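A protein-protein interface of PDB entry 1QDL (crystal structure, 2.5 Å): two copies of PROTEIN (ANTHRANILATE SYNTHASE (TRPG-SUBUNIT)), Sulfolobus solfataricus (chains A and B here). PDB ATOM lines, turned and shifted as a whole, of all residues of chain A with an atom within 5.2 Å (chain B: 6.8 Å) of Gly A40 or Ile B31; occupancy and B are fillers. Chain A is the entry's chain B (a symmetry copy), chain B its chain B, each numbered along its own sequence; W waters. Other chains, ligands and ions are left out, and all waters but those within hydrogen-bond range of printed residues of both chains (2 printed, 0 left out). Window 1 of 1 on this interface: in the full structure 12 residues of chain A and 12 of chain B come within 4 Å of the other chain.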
ATOM      1  N   ILE A  36      10.837  11.438   3.441  1.00  0.00           N
ATOM      2  CA  ILE A  36      10.774  10.265   2.591  1.00  0.00           C
ATOM      3  C   ILE A  36       9.984   9.150   3.278  1.00  0.00           C
ATOM      4  O   ILE A  36       9.989   9.044   4.510  1.00  0.00           O
ATOM      5  CB  ILE A  36      12.196   9.771   2.227  1.00  0.00           C
ATOM      6  CG1 ILE A  36      12.099   8.744   1.092  1.00  0.00           C
ATOM      7  CG2 ILE A  36      12.903   9.222   3.474  1.00  0.00           C
ATOM      8  CD1 ILE A  36      13.392   8.040   0.785  1.00  0.00           C
ATOM      9  N   SER A  37       9.291   8.343   2.474  1.00  0.00           N
ATOM     10  CA  SER A  37       8.480   7.238   2.982  1.00  0.00           C
ATOM     11  C   SER A  37       9.342   5.997   3.108  1.00  0.00           C
ATOM     12  O   SER A  37      10.403   5.903   2.489  1.00  0.00           O
ATOM     13  CB  SER A  37       7.287   6.973   2.044  1.00  0.00           C
ATOM     14  OG  SER A  37       7.530   5.921   1.121  1.00  0.00           O
ATOM     15  N   ILE A  38       8.899   5.047   3.918  1.00  0.00           N
ATOM     16  CA  ILE A  38       9.660   3.822   4.102  1.00  0.00           C
ATOM     17  C   ILE A  38       9.686   3.052   2.779  1.00  0.00           C
ATOM     18  O   ILE A  38      10.647   2.347   2.466  1.00  0.00           O
ATOM     19  CB  ILE A  38       9.040   2.971   5.225  1.00  0.00           C
ATOM     20  CG1 ILE A  38       9.798   1.661   5.370  1.00  0.00           C
ATOM     21  CG2 ILE A  38       7.584   2.727   4.941  1.00  0.00           C
ATOM     22  CD1 ILE A  38      10.352   1.474   6.755  1.00  0.00           C
ATOM     23  N   LYS A  39       8.631   3.204   1.987  1.00  0.00           N
ATOM     24  CA  LYS A  39       8.582   2.528   0.710  1.00  0.00           C
ATOM     25  C   LYS A  39       9.570   3.239  -0.198  1.00  0.00           C
ATOM     26  O   LYS A  39      10.316   2.598  -0.935  1.00  0.00           O
ATOM     27  CB  LYS A  39       7.177   2.594   0.130  1.00  0.00           C
ATOM     28  CG  LYS A  39       6.623   1.232  -0.234  1.00  0.00           C
ATOM     29  CD  LYS A  39       5.457   0.828   0.664  1.00  0.00           C
ATOM     30  CE  LYS A  39       4.847  -0.517   0.228  1.00  0.00           C
ATOM     31  NZ  LYS A  39       5.712  -1.692   0.572  1.00  0.00           N
ATOM     32  N   GLY A  40       9.584   4.566  -0.131  1.00  0.00           N
ATOM     33  CA  GLY A  40      10.505   5.338  -0.949  1.00  0.00           C
ATOM     34  C   GLY A  40      11.956   4.997  -0.638  1.00  0.00           C
ATOM     35  O   GLY A  40      12.816   4.992  -1.524  1.00  0.00           O
ATOM     36  N   ILE A  41      12.235   4.717   0.631  1.00  0.00           N
ATOM     37  CA  ILE A  41      13.582   4.367   1.049  1.00  0.00           C
ATOM     38  C   ILE A  41      13.896   3.045   0.373  1.00  0.00           C
ATOM     39  O   ILE A  41      14.964   2.859  -0.220  1.00  0.00           O
ATOM     40  CB  ILE A  41      13.662   4.192   2.586  1.00  0.00           C
ATOM     41  CG1 ILE A  41      13.623   5.559   3.274  1.00  0.00           C
ATOM     42  CG2 ILE A  41      14.943   3.458   2.973  1.00  0.00           C
ATOM     43  CD1 ILE A  41      13.762   5.482   4.779  1.00  0.00           C
ATOM     44  N   GLU A  42      12.939   2.131   0.466  1.00  0.00           N
ATOM     45  CA  GLU A  42      13.071   0.816  -0.137  1.00  0.00           C
ATOM     46  C   GLU A  42      13.434   0.958  -1.612  1.00  0.00           C
ATOM     47  O   GLU A  42      14.321   0.268  -2.108  1.00  0.00           O
ATOM     48  CB  GLU A  42      11.752   0.062  -0.015  1.00  0.00           C
ATOM     49  CG  GLU A  42      11.789  -1.147   0.905  1.00  0.00           C
ATOM     50  CD  GLU A  42      10.398  -1.621   1.291  1.00  0.00           C
ATOM     51  OE1 GLU A  42       9.511  -1.659   0.410  1.00  0.00           O
ATOM     52  OE2 GLU A  42      10.188  -1.955   2.477  1.00  0.00           O
ATOM     53  N   ARG A  43      12.750   1.868  -2.301  1.00  0.00           N
ATOM     54  CA  ARG A  43      12.968   2.104  -3.725  1.00  0.00           C
ATOM     55  C   ARG A  43      14.361   2.636  -4.058  1.00  0.00           C
ATOM     56  O   ARG A  43      14.872   2.419  -5.154  1.00  0.00           O
ATOM     57  CB  ARG A  43      11.895   3.058  -4.262  1.00  0.00           C
ATOM     58  CG  ARG A  43      11.677   2.978  -5.775  1.00  0.00           C
ATOM     59  CD  ARG A  43      10.323   3.551  -6.198  1.00  0.00           C
ATOM     60  NE  ARG A  43       9.248   3.114  -5.311  1.00  0.00           N
ATOM     61  CZ  ARG A  43       8.463   2.066  -5.550  1.00  0.00           C
ATOM     62  NH1 ARG A  43       8.635   1.352  -6.652  1.00  0.00           N
ATOM     63  NH2 ARG A  43       7.516   1.723  -4.685  1.00  0.00           N
ATOM     64  N   ILE A  44      14.982   3.339  -3.120  1.00  0.00           N
ATOM     65  CA  ILE A  44      16.322   3.861  -3.347  1.00  0.00           C
ATOM     66  C   ILE A  44      17.302   2.695  -3.197  1.00  0.00           C
ATOM     67  O   ILE A  44      18.355   2.648  -3.839  1.00  0.00           O
ATOM     68  CB  ILE A  44      16.652   4.939  -2.304  1.00  0.00           C
ATOM     69  CG1 ILE A  44      15.993   6.254  -2.702  1.00  0.00           C
ATOM     70  CG2 ILE A  44      18.163   5.079  -2.148  1.00  0.00           C
ATOM     71  CD1 ILE A  44      15.887   7.227  -1.568  1.00  0.00           C
ATOM     72  N   LEU B   5      17.107  12.371 -10.866  1.00  0.00           N
ATOM     73  CA  LEU B   5      16.005  11.886 -10.062  1.00  0.00           C
ATOM     74  C   LEU B   5      14.840  11.670 -11.013  1.00  0.00           C
ATOM     75  O   LEU B   5      14.486  12.568 -11.788  1.00  0.00           O
ATOM     76  CB  LEU B   5      15.611  12.902  -8.995  1.00  0.00           C
ATOM     77  CG  LEU B   5      14.320  12.522  -8.261  1.00  0.00           C
ATOM     78  CD1 LEU B   5      14.613  11.491  -7.192  1.00  0.00           C
ATOM     79  CD2 LEU B   5      13.704  13.748  -7.646  1.00  0.00           C
ATOM     80  N   ILE B   6      14.265  10.472 -10.967  1.00  0.00           N
ATOM     81  CA  ILE B   6      13.134  10.142 -11.818  1.00  0.00           C
ATOM     82  C   ILE B   6      11.926   9.904 -10.929  1.00  0.00           C
ATOM     83  O   ILE B   6      11.899   8.951 -10.149  1.00  0.00           O
ATOM     84  CB  ILE B   6      13.395   8.862 -12.652  1.00  0.00           C
ATOM     85  CG1 ILE B   6      14.678   9.007 -13.475  1.00  0.00           C
ATOM     86  CG2 ILE B   6      12.231   8.616 -13.603  1.00  0.00           C
ATOM     87  CD1 ILE B   6      15.232   7.687 -13.951  1.00  0.00           C
ATOM     88  N   ILE B   7      10.937  10.784 -11.028  1.00  0.00           N
ATOM     89  CA  ILE B   7       9.731  10.634 -10.232  1.00  0.00           C
ATOM     90  C   ILE B   7       8.828   9.645 -10.944  1.00  0.00           C
ATOM     91  O   ILE B   7       8.347   9.902 -12.047  1.00  0.00           O
ATOM     92  CB  ILE B   7       9.002  11.973 -10.064  1.00  0.00           C
ATOM     93  CG1 ILE B   7       9.729  12.805  -9.015  1.00  0.00           C
ATOM     94  CG2 ILE B   7       7.552  11.754  -9.625  1.00  0.00           C
ATOM     95  CD1 ILE B   7       9.524  14.278  -9.203  1.00  0.00           C
ATOM     96  N   ASP B   8       8.610   8.512 -10.289  1.00  0.00           N
ATOM     97  CA  ASP B   8       7.801   7.419 -10.812  1.00  0.00           C
ATOM     98  C   ASP B   8       6.318   7.567 -10.498  1.00  0.00           C
ATOM     99  O   ASP B   8       5.896   7.413  -9.345  1.00  0.00           O
ATOM    100  CB  ASP B   8       8.330   6.099 -10.232  1.00  0.00           C
ATOM    101  CG  ASP B   8       7.521   4.897 -10.665  1.00  0.00           C
ATOM    102  OD1 ASP B   8       6.789   5.006 -11.671  1.00  0.00           O
ATOM    103  OD2 ASP B   8       7.630   3.839  -9.997  1.00  0.00           O
ATOM    104  N   ASN B   9       5.528   7.864 -11.523  1.00  0.00           N
ATOM    105  CA  ASN B   9       4.089   7.994 -11.333  1.00  0.00           C
ATOM    106  C   ASN B   9       3.438   6.634 -11.523  1.00  0.00           C
ATOM    107  O   ASN B   9       2.582   6.466 -12.386  1.00  0.00           O
ATOM    108  CB  ASN B   9       3.521   8.996 -12.324  1.00  0.00           C
ATOM    109  CG  ASN B   9       3.925  10.406 -11.988  1.00  0.00           C
ATOM    110  OD1 ASN B   9       3.831  10.825 -10.834  1.00  0.00           O
ATOM    111  ND2 ASN B   9       4.396  11.145 -12.982  1.00  0.00           N
ATOM    112  N   VAL B  14       8.923   3.585 -16.678  1.00  0.00           N
ATOM    113  CA  VAL B  14       9.898   4.359 -15.933  1.00  0.00           C
ATOM    114  C   VAL B  14      11.309   3.777 -15.908  1.00  0.00           C
ATOM    115  O   VAL B  14      12.282   4.529 -15.965  1.00  0.00           O
ATOM    116  CB  VAL B  14       9.386   4.618 -14.485  1.00  0.00           C
ATOM    117  CG1 VAL B  14       9.228   3.309 -13.738  1.00  0.00           C
ATOM    118  CG2 VAL B  14      10.327   5.568 -13.760  1.00  0.00           C
ATOM    119  N   TYR B  15      11.439   2.457 -15.845  1.00  0.00           N
ATOM    120  CA  TYR B  15      12.776   1.864 -15.823  1.00  0.00           C
ATOM    121  C   TYR B  15      13.459   1.863 -17.181  1.00  0.00           C
ATOM    122  O   TYR B  15      14.654   1.593 -17.283  1.00  0.00           O
ATOM    123  CB  TYR B  15      12.728   0.459 -15.244  1.00  0.00           C
ATOM    124  CG  TYR B  15      12.561   0.523 -13.757  1.00  0.00           C
ATOM    125  CD1 TYR B  15      11.299   0.422 -13.179  1.00  0.00           C
ATOM    126  CD2 TYR B  15      13.648   0.794 -12.933  1.00  0.00           C
ATOM    127  CE1 TYR B  15      11.119   0.602 -11.813  1.00  0.00           C
ATOM    128  CE2 TYR B  15      13.481   0.975 -11.567  1.00  0.00           C
ATOM    129  CZ  TYR B  15      12.213   0.880 -11.008  1.00  0.00           C
ATOM    130  OH  TYR B  15      12.026   1.084  -9.655  1.00  0.00           O
ATOM    131  N   ILE B  29      17.916   7.842  -9.828  1.00  0.00           N
ATOM    132  CA  ILE B  29      17.222   7.498  -8.595  1.00  0.00           C
ATOM    133  C   ILE B  29      15.740   7.552  -8.922  1.00  0.00           C
ATOM    134  O   ILE B  29      15.209   8.603  -9.287  1.00  0.00           O
ATOM    135  CB  ILE B  29      17.515   8.482  -7.457  1.00  0.00           C
ATOM    136  CG1 ILE B  29      18.826   8.105  -6.781  1.00  0.00           C
ATOM    137  CG2 ILE B  29      16.420   8.415  -6.411  1.00  0.00           C
ATOM    138  CD1 ILE B  29      19.822   9.223  -6.763  1.00  0.00           C
ATOM    139  N   VAL B  30      15.087   6.401  -8.804  1.00  0.00           N
ATOM    140  CA  VAL B  30      13.664   6.277  -9.095  1.00  0.00           C
ATOM    141  C   VAL B  30      12.845   6.244  -7.812  1.00  0.00           C
ATOM    142  O   VAL B  30      13.035   5.366  -6.965  1.00  0.00           O
ATOM    143  CB  VAL B  30      13.369   4.979  -9.900  1.00  0.00           C
ATOM    144  CG1 VAL B  30      11.925   4.984 -10.391  1.00  0.00           C
ATOM    145  CG2 VAL B  30      14.337   4.854 -11.067  1.00  0.00           C
ATOM    146  N   ILE B  31      11.936   7.201  -7.670  1.00  0.00           N
ATOM    147  CA  ILE B  31      11.081   7.269  -6.490  1.00  0.00           C
ATOM    148  C   ILE B  31       9.698   7.762  -6.931  1.00  0.00           C
ATOM    149  O   ILE B  31       9.590   8.628  -7.803  1.00  0.00           O
ATOM    150  CB  ILE B  31      11.706   8.199  -5.401  1.00  0.00           C
ATOM    151  CG1 ILE B  31      10.800   8.259  -4.173  1.00  0.00           C
ATOM    152  CG2 ILE B  31      11.935   9.579  -5.958  1.00  0.00           C
ATOM    153  CD1 ILE B  31      11.471   7.782  -2.921  1.00  0.00           C
ATOM    154  N   ARG B  32       8.649   7.205  -6.334  1.00  0.00           N
ATOM    155  CA  ARG B  32       7.280   7.550  -6.710  1.00  0.00           C
ATOM    156  C   ARG B  32       6.739   8.878  -6.225  1.00  0.00           C
ATOM    157  O   ARG B  32       7.089   9.353  -5.146  1.00  0.00           O
ATOM    158  CB  ARG B  32       6.346   6.425  -6.293  1.00  0.00           C
ATOM    159  CG  ARG B  32       6.800   5.105  -6.860  1.00  0.00           C
ATOM    160  CD  ARG B  32       5.797   4.025  -6.621  1.00  0.00           C
ATOM    161  NE  ARG B  32       5.614   3.196  -7.803  1.00  0.00           N
ATOM    162  CZ  ARG B  32       5.128   1.960  -7.772  1.00  0.00           C
ATOM    163  NH1 ARG B  32       4.778   1.407  -6.616  1.00  0.00           N
ATOM    164  NH2 ARG B  32       4.973   1.285  -8.899  1.00  0.00           N
ATOM    165  N   ASN B  33       5.861   9.456  -7.044  1.00  0.00           N
ATOM    166  CA  ASN B  33       5.247  10.748  -6.785  1.00  0.00           C
ATOM    167  C   ASN B  33       4.743  11.002  -5.364  1.00  0.00           C
ATOM    168  O   ASN B  33       4.490  12.146  -4.994  1.00  0.00           O
ATOM    169  CB  ASN B  33       4.117  10.992  -7.793  1.00  0.00           C
ATOM    170  CG  ASN B  33       2.898  10.105  -7.556  1.00  0.00           C
ATOM    171  OD1 ASN B  33       2.532   9.794  -6.417  1.00  0.00           O
ATOM    172  ND2 ASN B  33       2.256   9.702  -8.645  1.00  0.00           N
ATOM    173  N   ASP B  34       4.591   9.955  -4.565  1.00  0.00           N
ATOM    174  CA  ASP B  34       4.104  10.146  -3.209  1.00  0.00           C
ATOM    175  C   ASP B  34       5.009   9.516  -2.146  1.00  0.00           C
ATOM    176  O   ASP B  34       4.559   9.221  -1.036  1.00  0.00           O
ATOM    177  CB  ASP B  34       2.660   9.610  -3.090  1.00  0.00           C
ATOM    178  CG  ASP B  34       2.559   8.096  -3.274  1.00  0.00           C
ATOM    179  OD1 ASP B  34       1.511   7.513  -2.888  1.00  0.00           O
ATOM    180  OD2 ASP B  34       3.523   7.495  -3.801  1.00  0.00           O
ATOM    181  N   GLU B  35       6.284   9.321  -2.471  1.00  0.00           N
ATOM    182  CA  GLU B  35       7.199   8.712  -1.509  1.00  0.00           C
ATOM    183  C   GLU B  35       8.260   9.666  -1.008  1.00  0.00           C
ATOM    184  O   GLU B  35       9.032   9.334  -0.109  1.00  0.00           O
ATOM    185  CB  GLU B  35       7.882   7.499  -2.119  1.00  0.00           C
ATOM    186  CG  GLU B  35       6.950   6.378  -2.449  1.00  0.00           C
ATOM    187  CD  GLU B  35       7.660   5.288  -3.192  1.00  0.00           C
ATOM    188  OE1 GLU B  35       8.518   5.616  -4.032  1.00  0.00           O
ATOM    189  OE2 GLU B  35       7.371   4.109  -2.935  1.00  0.00           O
ATOM    190  N   ILE B  36       8.310  10.851  -1.596  1.00  0.00           N
ATOM    191  CA  ILE B  36       9.295  11.833  -1.186  1.00  0.00           C
ATOM    192  C   ILE B  36       8.689  13.236  -1.207  1.00  0.00           C
ATOM    193  O   ILE B  36       7.800  13.526  -2.016  1.00  0.00           O
ATOM    194  CB  ILE B  36      10.545  11.773  -2.098  1.00  0.00           C
ATOM    195  CG1 ILE B  36      11.677  12.586  -1.458  1.00  0.00           C
ATOM    196  CG2 ILE B  36      10.192  12.249  -3.514  1.00  0.00           C
ATOM    197  CD1 ILE B  36      12.879  12.773  -2.342  1.00  0.00           C
ATOM    198  N   ILE B  41      13.414  16.225  -1.892  1.00  0.00           N
ATOM    199  CA  ILE B  41      13.987  16.176  -3.226  1.00  0.00           C
ATOM    200  C   ILE B  41      15.106  17.201  -3.234  1.00  0.00           C
ATOM    201  O   ILE B  41      16.225  16.934  -3.686  1.00  0.00           O
ATOM    202  CB  ILE B  41      12.934  16.553  -4.300  1.00  0.00           C
ATOM    203  CG1 ILE B  41      11.949  15.398  -4.497  1.00  0.00           C
ATOM    204  CG2 ILE B  41      13.618  16.880  -5.624  1.00  0.00           C
ATOM    205  CD1 ILE B  41      10.922  15.659  -5.579  1.00  0.00           C
ATOM    206  N   ILE B  44      18.258  16.030  -1.766  1.00  0.00           N
ATOM    207  CA  ILE B  44      19.026  15.071  -2.546  1.00  0.00           C
ATOM    208  C   ILE B  44      19.856  15.862  -3.561  1.00  0.00           C
ATOM    209  O   ILE B  44      20.958  15.462  -3.948  1.00  0.00           O
ATOM    210  CB  ILE B  44      18.081  14.121  -3.296  1.00  0.00           C
ATOM    211  CG1 ILE B  44      17.573  13.047  -2.340  1.00  0.00           C
ATOM    212  CG2 ILE B  44      18.784  13.521  -4.509  1.00  0.00           C
ATOM    213  CD1 ILE B  44      16.343  12.351  -2.836  1.00  0.00           C
HETATM  214  O   HOH W   1      16.230   4.030  -7.449  1.00  0.00           O
HETATM  215  O   HOH W   2      14.261   1.480  -8.060  1.00  0.00           O
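O of Glu B35 is in hydrogen-bond range of N of Ser A37 (2.8 Å).
The side-chain carboxylate (OE1) of Glu B35 lies within salt-bridge range of the guanidinium group (NE) of Arg A43, at 2.9 Å.
The guanidinium group of Arg B32 lies close to the guanidinium group of Arg A43 (3.4 Å).
Among the printed residues, merely in contact across the chains: Arg A43 with Val B30 (3.0 Å), Gly A40 with Ile B31 (3.3 Å), Ile A36 with Glu B35 (3.3 Å), Lys A39 with Glu B35 (3.4 Å), Gly A40 with Glu B35 (3.6 Å) and Arg A43 with Ile B31 (3.8 Å).
Hydrophobic or aromatic side chains of chain B within 4 Å of the printed part of chain A: Ile B31.
Of the 9 printed residues of chain A, 5 touch a printed residue of chain B.
Hydrophobic or aromatic side chains of chain A within 4 Å of the printed part of chain B: Ile A36.
Water W2 lies within hydrogen-bond range of the side-chain hydroxyl (OH) of Tyr B15 (2.8 Å) and the backbone carbonyl oxygen (O) of Arg A43 (3.1 Å).
Water W1 lies within hydrogen-bond range of the backbone NH of Val B30 (3.0 Å) and the backbone carbonyl oxygen of Arg A43 (3.1 Å).
Positions printed for both chains: 36, 41 and 44.
Of the 9 pairs that touch across the chains among the printed residues, none has its exchanged pair printed and touching as well.
OG of Ser A37 sits at hydrogen-bond distance from N of Lys A39 (3.1 Å).
The backbone carbonyl oxygen of Ile B6 sits at hydrogen-bond distance from the backbone NH of Ile B31.
OG of Ser A37 sits at hydrogen-bond distance from N of Gly A40 (2.8 Å).
The side-chain carboxylate (OE1) of Glu B35 lies within hydrogen-bond range of the backbone NH (N) of Arg B32, 2.8 Å away.
The side-chain amino group (NZ) of Lys A39 is in salt-bridge range of the side-chain carboxylate (OE1) of Glu A42, 3.8 Å away.
OD2 of Asp B8 lies within salt-bridge range of NE of Arg B32, at 3.0 Å.
Printed residues of chain B within 4 Å of Ser A37: Glu B35 (2.8 Å).
Of the printed residues of chain B, Lys A39 touches Glu B35 (3.4 Å).
Of chain B, only Ile B31 (3.3 Å) and Glu B35 (3.6 Å) come within 4 Å of Gly A40.
Of chain A, only Gly A40 and Arg A43 come within 4 Å of Ile B31.
Of the printed residues of chain A, Arg B32 touches Arg A43 (3.4 Å).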
